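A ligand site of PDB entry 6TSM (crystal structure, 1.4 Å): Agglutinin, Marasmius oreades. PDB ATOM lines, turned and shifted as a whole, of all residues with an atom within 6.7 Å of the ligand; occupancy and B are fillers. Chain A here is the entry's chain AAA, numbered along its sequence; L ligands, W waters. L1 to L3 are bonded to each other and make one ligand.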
ATOM      1  N   HIS A   9      -0.708  -9.459  20.191  1.00  0.00           N
ATOM      2  CA  HIS A   9      -1.168 -10.829  20.463  1.00  0.00           C
ATOM      3  C   HIS A   9      -0.913 -11.686  19.229  1.00  0.00           C
ATOM      4  O   HIS A   9      -1.393 -11.310  18.171  1.00  0.00           O
ATOM      5  CB  HIS A   9      -2.638 -10.810  20.832  1.00  0.00           C
ATOM      6  CG  HIS A   9      -3.145 -12.082  21.435  1.00  0.00           C
ATOM      7  ND1 HIS A   9      -4.089 -12.883  20.809  1.00  0.00           N
ATOM      8  CD2 HIS A   9      -2.783 -12.744  22.560  1.00  0.00           C
ATOM      9  CE1 HIS A   9      -4.319 -13.950  21.551  1.00  0.00           C
ATOM     10  NE2 HIS A   9      -3.557 -13.881  22.631  1.00  0.00           N
ATOM     11  N   ASP A  20       2.556 -18.033  23.935  1.00  0.00           N
ATOM     12  CA  ASP A  20       2.270 -17.929  25.370  1.00  0.00           C
ATOM     13  C   ASP A  20       3.563 -18.183  26.136  1.00  0.00           C
ATOM     14  O   ASP A  20       4.203 -19.210  25.879  1.00  0.00           O
ATOM     15  CB  ASP A  20       1.151 -18.896  25.765  1.00  0.00           C
ATOM     16  CG  ASP A  20       0.694 -18.822  27.207  1.00  0.00           C
ATOM     17  OD1 ASP A  20       1.506 -19.126  28.066  1.00  0.00           O
ATOM     18  OD2 ASP A  20      -0.540 -18.586  27.431  1.00  0.00           O
ATOM     19  N   LEU A  21       3.950 -17.278  27.001  1.00  0.00           N
ATOM     20  CA  LEU A  21       5.053 -17.568  27.951  1.00  0.00           C
ATOM     21  C   LEU A  21       4.490 -18.358  29.121  1.00  0.00           C
ATOM     22  O   LEU A  21       3.677 -17.772  29.907  1.00  0.00           O
ATOM     23  CB  LEU A  21       5.671 -16.257  28.437  1.00  0.00           C
ATOM     24  CG  LEU A  21       6.858 -16.407  29.413  1.00  0.00           C
ATOM     25  CD1 LEU A  21       8.006 -17.148  28.778  1.00  0.00           C
ATOM     26  CD2 LEU A  21       7.318 -15.048  29.913  1.00  0.00           C
ATOM     27  N   LYS A  22       4.904 -19.613  29.278  1.00  0.00           N
ATOM     28  CA  LYS A  22       4.176 -20.557  30.153  1.00  0.00           C
ATOM     29  C   LYS A  22       4.153 -20.001  31.603  1.00  0.00           C
ATOM     30  O   LYS A  22       5.242 -19.721  32.171  1.00  0.00           O
ATOM     31  CB  LYS A  22       4.786 -21.955  30.106  1.00  0.00           C
ATOM     32  CG  LYS A  22       3.834 -23.047  30.509  1.00  0.00           C
ATOM     33  CD  LYS A  22       4.333 -24.444  30.306  1.00  0.00           C
ATOM     34  CE  LYS A  22       3.323 -25.477  30.780  1.00  0.00           C
ATOM     35  NZ  LYS A  22       3.683 -26.851  30.330  1.00  0.00           N
ATOM     36  N   ASP A  23       2.946 -19.902  32.168  1.00  0.00           N
ATOM     37  CA  ASP A  23       2.670 -19.431  33.556  1.00  0.00           C
ATOM     38  C   ASP A  23       3.183 -17.980  33.743  1.00  0.00           C
ATOM     39  O   ASP A  23       3.207 -17.520  34.890  1.00  0.00           O
ATOM     40  CB  ASP A  23       3.294 -20.364  34.578  1.00  0.00           C
ATOM     41  CG  ASP A  23       2.575 -20.333  35.915  1.00  0.00           C
ATOM     42  OD1 ASP A  23       1.351 -20.121  35.920  1.00  0.00           O
ATOM     43  OD2 ASP A  23       3.274 -20.412  36.948  1.00  0.00           O
ATOM     44  N   GLY A  24       3.532 -17.303  32.666  1.00  0.00           N
ATOM     45  CA  GLY A  24       4.042 -15.930  32.734  1.00  0.00           C
ATOM     46  C   GLY A  24       5.386 -15.847  33.481  1.00  0.00           C
ATOM     47  O   GLY A  24       5.727 -14.768  33.956  1.00  0.00           O
ATOM     48  N   VAL A  33       5.088 -21.433  24.364  1.00  0.00           N
ATOM     49  CA  VAL A  33       4.235 -22.553  23.919  1.00  0.00           C
ATOM     50  C   VAL A  33       3.001 -21.974  23.192  1.00  0.00           C
ATOM     51  O   VAL A  33       2.655 -20.808  23.425  1.00  0.00           O
ATOM     52  CB  VAL A  33       3.810 -23.431  25.104  1.00  0.00           C
ATOM     53  CG1 VAL A  33       5.001 -24.123  25.748  1.00  0.00           C
ATOM     54  CG2 VAL A  33       3.023 -22.646  26.142  1.00  0.00           C
ATOM     55  N   TRP A  35      -1.015 -21.781  23.030  1.00  0.00           N
ATOM     56  CA  TRP A  35      -2.087 -21.858  24.057  1.00  0.00           C
ATOM     57  C   TRP A  35      -3.339 -21.198  23.520  1.00  0.00           C
ATOM     58  O   TRP A  35      -3.229 -20.170  22.849  1.00  0.00           O
ATOM     59  CB  TRP A  35      -1.617 -21.197  25.385  1.00  0.00           C
ATOM     60  CG  TRP A  35      -2.293 -21.735  26.602  1.00  0.00           C
ATOM     61  CD1 TRP A  35      -3.555 -21.474  27.031  1.00  0.00           C
ATOM     62  CD2 TRP A  35      -1.739 -22.681  27.539  1.00  0.00           C
ATOM     63  NE1 TRP A  35      -3.826 -22.188  28.186  1.00  0.00           N
ATOM     64  CE2 TRP A  35      -2.737 -22.951  28.505  1.00  0.00           C
ATOM     65  CE3 TRP A  35      -0.509 -23.360  27.624  1.00  0.00           C
ATOM     66  CZ2 TRP A  35      -2.533 -23.864  29.534  1.00  0.00           C
ATOM     67  CZ3 TRP A  35      -0.304 -24.244  28.653  1.00  0.00           C
ATOM     68  CH2 TRP A  35      -1.311 -24.501  29.591  1.00  0.00           C
ATOM     69  N   GLN A  36      -4.483 -21.677  23.901  1.00  0.00           N
ATOM     70  CA  GLN A  36      -5.756 -21.072  23.450  1.00  0.00           C
ATOM     71  C   GLN A  36      -5.967 -19.720  24.162  1.00  0.00           C
ATOM     72  O   GLN A  36      -5.278 -19.445  25.162  1.00  0.00           O
ATOM     73  CB  GLN A  36      -6.944 -22.025  23.717  1.00  0.00           C
ATOM     74  CG  GLN A  36      -7.241 -22.281  25.163  1.00  0.00           C
ATOM     75  CD  GLN A  36      -8.448 -23.178  25.345  1.00  0.00           C
ATOM     76  OE1 GLN A  36      -9.559 -22.846  24.939  1.00  0.00           O
ATOM     77  NE2 GLN A  36      -8.212 -24.360  25.861  1.00  0.00           N
ATOM     78  N   PHE A  37      -6.894 -18.928  23.665  1.00  0.00           N
ATOM     79  CA  PHE A  37      -7.044 -17.546  24.129  1.00  0.00           C
ATOM     80  C   PHE A  37      -8.513 -17.150  24.069  1.00  0.00           C
ATOM     81  O   PHE A  37      -9.315 -17.869  23.484  1.00  0.00           O
ATOM     82  CB  PHE A  37      -6.157 -16.613  23.289  1.00  0.00           C
ATOM     83  CG  PHE A  37      -6.419 -16.651  21.805  1.00  0.00           C
ATOM     84  CD1 PHE A  37      -7.344 -15.790  21.222  1.00  0.00           C
ATOM     85  CD2 PHE A  37      -5.673 -17.469  20.973  1.00  0.00           C
ATOM     86  CE1 PHE A  37      -7.546 -15.801  19.851  1.00  0.00           C
ATOM     87  CE2 PHE A  37      -5.883 -17.465  19.601  1.00  0.00           C
ATOM     88  CZ  PHE A  37      -6.810 -16.632  19.047  1.00  0.00           C
ATOM     89  N   THR A  38      -8.853 -16.119  24.799  1.00  0.00           N
ATOM     90  CA  THR A  38     -10.217 -15.549  24.786  1.00  0.00           C
ATOM     91  C   THR A  38     -10.157 -14.158  24.161  1.00  0.00           C
ATOM     92  O   THR A  38      -9.550 -13.263  24.715  1.00  0.00           O
ATOM     93  CB  THR A  38     -10.815 -15.507  26.193  1.00  0.00           C
ATOM     94  OG1 THR A  38     -10.602 -16.801  26.810  1.00  0.00           O
ATOM     95  CG2 THR A  38     -12.286 -15.167  26.190  1.00  0.00           C
ATOM     96  N   PRO A  39     -10.791 -13.948  23.006  1.00  0.00           N
ATOM     97  CA  PRO A  39     -10.843 -12.603  22.402  1.00  0.00           C
ATOM     98  C   PRO A  39     -11.533 -11.588  23.331  1.00  0.00           C
ATOM     99  O   PRO A  39     -12.385 -11.993  24.100  1.00  0.00           O
ATOM    100  CB  PRO A  39     -11.679 -12.800  21.111  1.00  0.00           C
ATOM    101  CG  PRO A  39     -11.634 -14.325  20.854  1.00  0.00           C
ATOM    102  CD  PRO A  39     -11.511 -14.949  22.234  1.00  0.00           C
ATOM    103  N   THR A  41     -10.415 -10.012  25.864  1.00  0.00           N
ATOM    104  CA  THR A  41      -9.884 -10.004  27.214  1.00  0.00           C
ATOM    105  C   THR A  41      -8.440  -9.530  27.171  1.00  0.00           C
ATOM    106  O   THR A  41      -7.840  -9.547  26.054  1.00  0.00           O
ATOM    107  CB  THR A  41      -9.954 -11.394  27.881  1.00  0.00           C
ATOM    108  OG1 THR A  41      -9.000 -12.272  27.234  1.00  0.00           O
ATOM    109  CG2 THR A  41     -11.323 -12.006  27.834  1.00  0.00           C
ATOM    110  N   ILE A  42      -7.862  -9.306  28.328  1.00  0.00           N
ATOM    111  CA  ILE A  42      -6.392  -9.325  28.503  1.00  0.00           C
ATOM    112  C   ILE A  42      -5.944 -10.787  28.627  1.00  0.00           C
ATOM    113  O   ILE A  42      -6.374 -11.463  29.605  1.00  0.00           O
ATOM    114  CB  ILE A  42      -5.977  -8.502  29.723  1.00  0.00           C
ATOM    115  CG1 ILE A  42      -6.344  -7.015  29.557  1.00  0.00           C
ATOM    116  CG2 ILE A  42      -4.512  -8.682  30.021  1.00  0.00           C
ATOM    117  CD1 ILE A  42      -5.706  -6.361  28.382  1.00  0.00           C
ATOM    118  N   ASN A  43      -5.229 -11.280  27.621  1.00  0.00           N
ATOM    119  CA  ASN A  43      -4.587 -12.600  27.679  1.00  0.00           C
ATOM    120  C   ASN A  43      -3.202 -12.441  28.334  1.00  0.00           C
ATOM    121  O   ASN A  43      -2.230 -12.054  27.621  1.00  0.00           O
ATOM    122  CB  ASN A  43      -4.527 -13.263  26.294  1.00  0.00           C
ATOM    123  CG  ASN A  43      -5.909 -13.660  25.798  1.00  0.00           C
ATOM    124  OD1 ASN A  43      -6.449 -14.665  26.214  1.00  0.00           O
ATOM    125  ND2 ASN A  43      -6.497 -12.847  24.926  1.00  0.00           N
ATOM    126  N   TRP A  44      -3.146 -12.611  29.651  1.00  0.00           N
ATOM    127  CA  TRP A  44      -2.089 -12.065  30.521  1.00  0.00           C
ATOM    128  C   TRP A  44      -0.703 -12.542  30.080  1.00  0.00           C
ATOM    129  O   TRP A  44       0.269 -11.803  30.324  1.00  0.00           O
ATOM    130  CB  TRP A  44      -2.380 -12.456  31.975  1.00  0.00           C
ATOM    131  CG  TRP A  44      -3.385 -11.591  32.623  1.00  0.00           C
ATOM    132  CD1 TRP A  44      -4.741 -11.784  32.705  1.00  0.00           C
ATOM    133  CD2 TRP A  44      -3.146 -10.276  33.130  1.00  0.00           C
ATOM    134  NE1 TRP A  44      -5.330 -10.712  33.286  1.00  0.00           N
ATOM    135  CE2 TRP A  44      -4.381  -9.760  33.556  1.00  0.00           C
ATOM    136  CE3 TRP A  44      -2.013  -9.486  33.247  1.00  0.00           C
ATOM    137  CZ2 TRP A  44      -4.495  -8.512  34.156  1.00  0.00           C
ATOM    138  CZ3 TRP A  44      -2.126  -8.252  33.847  1.00  0.00           C
ATOM    139  CH2 TRP A  44      -3.353  -7.765  34.273  1.00  0.00           C
ATOM    140  N   HIS A  45      -0.579 -13.789  29.607  1.00  0.00           N
ATOM    141  CA  HIS A  45       0.784 -14.370  29.316  1.00  0.00           C
ATOM    142  C   HIS A  45       1.095 -14.320  27.823  1.00  0.00           C
ATOM    143  O   HIS A  45       2.150 -14.858  27.440  1.00  0.00           O
ATOM    144  CB  HIS A  45       0.883 -15.796  29.857  1.00  0.00           C
ATOM    145  CG  HIS A  45       0.561 -15.910  31.301  1.00  0.00           C
ATOM    146  ND1 HIS A  45       0.136 -17.093  31.867  1.00  0.00           N
ATOM    147  CD2 HIS A  45       0.687 -15.024  32.322  1.00  0.00           C
ATOM    148  CE1 HIS A  45      -0.068 -16.916  33.167  1.00  0.00           C
ATOM    149  NE2 HIS A  45       0.248 -15.676  33.476  1.00  0.00           N
ATOM    150  N   GLN A  46       0.306 -13.585  27.037  1.00  0.00           N
ATOM    151  CA  GLN A  46       0.311 -13.724  25.546  1.00  0.00           C
ATOM    152  C   GLN A  46       0.451 -12.357  24.886  1.00  0.00           C
ATOM    153  O   GLN A  46       0.153 -12.263  23.697  1.00  0.00           O
ATOM    154  CB  GLN A  46      -0.969 -14.400  25.075  1.00  0.00           C
ATOM    155  CG  GLN A  46      -1.189 -15.772  25.700  1.00  0.00           C
ATOM    156  CD  GLN A  46      -2.469 -16.441  25.236  1.00  0.00           C
ATOM    157  OE1 GLN A  46      -3.302 -15.839  24.515  1.00  0.00           O
ATOM    158  NE2 GLN A  46      -2.675 -17.675  25.675  1.00  0.00           N
ATOM    159  N   PHE A  66       4.036  -9.236  30.544  1.00  0.00           N
ATOM    160  CA  PHE A  66       3.804  -9.651  31.935  1.00  0.00           C
ATOM    161  C   PHE A  66       5.158  -9.915  32.638  1.00  0.00           C
ATOM    162  O   PHE A  66       5.364  -9.363  33.713  1.00  0.00           O
ATOM    163  CB  PHE A  66       2.908 -10.890  31.973  1.00  0.00           C
ATOM    164  CG  PHE A  66       2.555 -11.365  33.358  1.00  0.00           C
ATOM    165  CD1 PHE A  66       1.552 -10.754  34.094  1.00  0.00           C
ATOM    166  CD2 PHE A  66       3.265 -12.390  33.957  1.00  0.00           C
ATOM    167  CE1 PHE A  66       1.240 -11.203  35.365  1.00  0.00           C
ATOM    168  CE2 PHE A  66       2.964 -12.804  35.249  1.00  0.00           C
ATOM    169  CZ  PHE A  66       1.930 -12.235  35.929  1.00  0.00           C
ATOM    170  N   ASP A 131      -2.998 -27.034  24.376  1.00  0.00           N
ATOM    171  CA  ASP A 131      -2.449 -26.048  25.339  1.00  0.00           C
ATOM    172  C   ASP A 131      -1.092 -26.548  25.839  1.00  0.00           C
ATOM    173  O   ASP A 131      -1.025 -27.668  26.398  1.00  0.00           O
ATOM    174  CB  ASP A 131      -3.392 -25.808  26.497  1.00  0.00           C
ATOM    175  CG  ASP A 131      -4.651 -25.069  26.107  1.00  0.00           C
ATOM    176  OD1 ASP A 131      -4.642 -24.417  25.038  1.00  0.00           O
ATOM    177  OD2 ASP A 131      -5.645 -25.222  26.810  1.00  0.00           O
HETATM  178  C1  LIG L   1      -5.547 -17.491  32.690  1.00  0.00           C
HETATM  179  C2  LIG L   1      -6.784 -17.706  33.550  1.00  0.00           C
HETATM  180  C3  LIG L   1      -6.432 -17.677  35.027  1.00  0.00           C
HETATM  181  C4  LIG L   1      -5.635 -16.437  35.365  1.00  0.00           C
HETATM  182  C5  LIG L   1      -4.412 -16.321  34.464  1.00  0.00           C
HETATM  183  C6  LIG L   1      -3.626 -15.095  34.746  1.00  0.00           C
HETATM  184  O1  LIG L   1      -7.371 -18.959  33.219  1.00  0.00           O
HETATM  185  O2  LIG L   1      -7.654 -17.730  35.835  1.00  0.00           O
HETATM  186  O3  LIG L   1      -6.451 -15.247  35.217  1.00  0.00           O
HETATM  187  O4  LIG L   1      -4.851 -16.275  33.085  1.00  0.00           O
HETATM  188  C1  LG2 L   2      -2.626 -19.540  32.897  1.00  0.00           C
HETATM  189  C2  LG2 L   2      -3.540 -18.625  32.102  1.00  0.00           C
HETATM  190  C3  LG2 L   2      -3.745 -19.131  30.694  1.00  0.00           C
HETATM  191  C4  LG2 L   2      -2.424 -19.440  30.010  1.00  0.00           C
HETATM  192  C5  LG2 L   2      -1.590 -20.366  30.933  1.00  0.00           C
HETATM  193  C6  LG2 L   2      -0.221 -20.759  30.336  1.00  0.00           C
HETATM  194  O1  LG2 L   2      -2.317 -18.926  34.077  1.00  0.00           O
HETATM  195  O2  LG2 L   2      -4.798 -18.565  32.795  1.00  0.00           O
HETATM  196  O3  LG2 L   2      -4.527 -18.148  29.954  1.00  0.00           O
HETATM  197  O4  LG2 L   2      -1.699 -18.227  29.719  1.00  0.00           O
HETATM  198  O5  LG2 L   2      -1.391 -19.726  32.191  1.00  0.00           O
HETATM  199  O6  LG2 L   2       0.710 -19.695  30.463  1.00  0.00           O
HETATM  200  C1  LG3 L   3      -4.928 -18.478  28.714  1.00  0.00           C
HETATM  201  C2  LG3 L   3      -5.828 -17.412  28.051  1.00  0.00           C
HETATM  202  C3  LG3 L   3      -7.219 -17.456  28.668  1.00  0.00           C
HETATM  203  C4  LG3 L   3      -7.751 -18.885  28.601  1.00  0.00           C
HETATM  204  C5  LG3 L   3      -6.767 -19.803  29.311  1.00  0.00           C
HETATM  205  C6  LG3 L   3      -7.219 -21.247  29.330  1.00  0.00           C
HETATM  206  O1  LG3 L   3      -5.280 -16.132  28.226  1.00  0.00           O
HETATM  207  O2  LG3 L   3      -8.074 -16.570  27.972  1.00  0.00           O
HETATM  208  O3  LG3 L   3      -7.934 -19.299  27.256  1.00  0.00           O
HETATM  209  O4  LG3 L   3      -5.535 -19.735  28.602  1.00  0.00           O
HETATM  210  O5  LG3 L   3      -6.272 -22.072  30.060  1.00  0.00           O
HETATM  211  O   HOH W   1      -6.040 -24.731  29.598  1.00  0.00           O
HETATM  212  O   HOH W   2      -7.405 -14.302  32.731  1.00  0.00           O
HETATM  213  O   HOH W   3      -7.234 -16.777  38.383  1.00  0.00           O
HETATM  214  O   HOH W   4      -5.459 -14.435  30.588  1.00  0.00           O
HETATM  215  O   HOH W   5      -2.587 -15.726  29.031  1.00  0.00           O
HETATM  216  O   HOH W   6      -6.123 -21.463  32.768  1.00  0.00           O
HETATM  217  O   HOH W   7      -9.446 -18.730  31.429  1.00  0.00           O
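Leu 21 touches the ligand.
CA of Lys 22 touches O6 of LG2 L2 (3.6 Å).
Phe 37 touches the ligand.
NE2 of Gln 46 touches C1 of LG3 L3 (3.9 Å).
Hydrophobic or aromatic side chains within 4 Å of the ligand: Trp 35 and His 45.
O of Val 33 lies within hydrogen-bond range of N of Asp 20.
The side-chain amide nitrogen (ND2) of Asn 43 lies within hydrogen-bond range of the backbone carbonyl oxygen (O) of Thr 38 (3.1 Å).
ND2 of Asn 43 lies within hydrogen-bond range of OG1 of Thr 41 (3.5 Å).
The backbone NH (N) of Leu 21 sits at hydrogen-bond distance from the backbone carbonyl oxygen (O) of His 45.
A ring nitrogen (ND1) of His 45 is in hydrogen-bond range of the backbone NH (N) of Gly 24 (3.5 Å).
O of Gln 36 is in hydrogen-bond range of NE2 of Gln 46.
NE2 of Gln 36 sits at hydrogen-bond distance from OD2 of Asp 131, at 2.9 Å.
The side-chain amide oxygen of Gln 46 sits at hydrogen-bond distance from a ring nitrogen (NE2) of His 9 (2.7 Å).
The side-chain carboxylate (OD2) of Asp 20 sits at hydrogen-bond distance from an oxygen (O4) of LG2 L2, at 2.6 Å.
An oxygen (O1) of LG3 L3 sits at hydrogen-bond distance from the side-chain amide oxygen (OD1) of Asn 43.
An oxygen (O2) of LG3 L3 is in hydrogen-bond range of the backbone NH of Thr 38.
An oxygen (O2) of LG3 L3 sits at hydrogen-bond distance from the side-chain hydroxyl of Thr 38.
N of Asp 23 is in hydrogen-bond range of O6 of LG2 L2.
ND1 of His 45 is in hydrogen-bond range of O6 of LG2 L2, 3.0 Å away.
O4 of LG3 L3 sits at hydrogen-bond distance from NE1 of Trp 35 (3.0 Å).
The backbone carbonyl oxygen (O) of Gln 36 sits at hydrogen-bond distance from an oxygen (O3) of LG3 L3.
Water W1 lies within hydrogen-bond range of an oxygen (O5) of LG3 L3 (2.7 Å) and the side-chain carboxylate of Asp 131 (2.9 Å).
Water W5 lies within hydrogen-bond range of O4 of LG2 L2, N of His 45 and N of Trp 44.
Water W4 lies within hydrogen-bond range of O1 of LG3 L3 (2.9 Å), N of Trp 44 (3.1 Å) and O of Ile 42 (3.3 Å).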
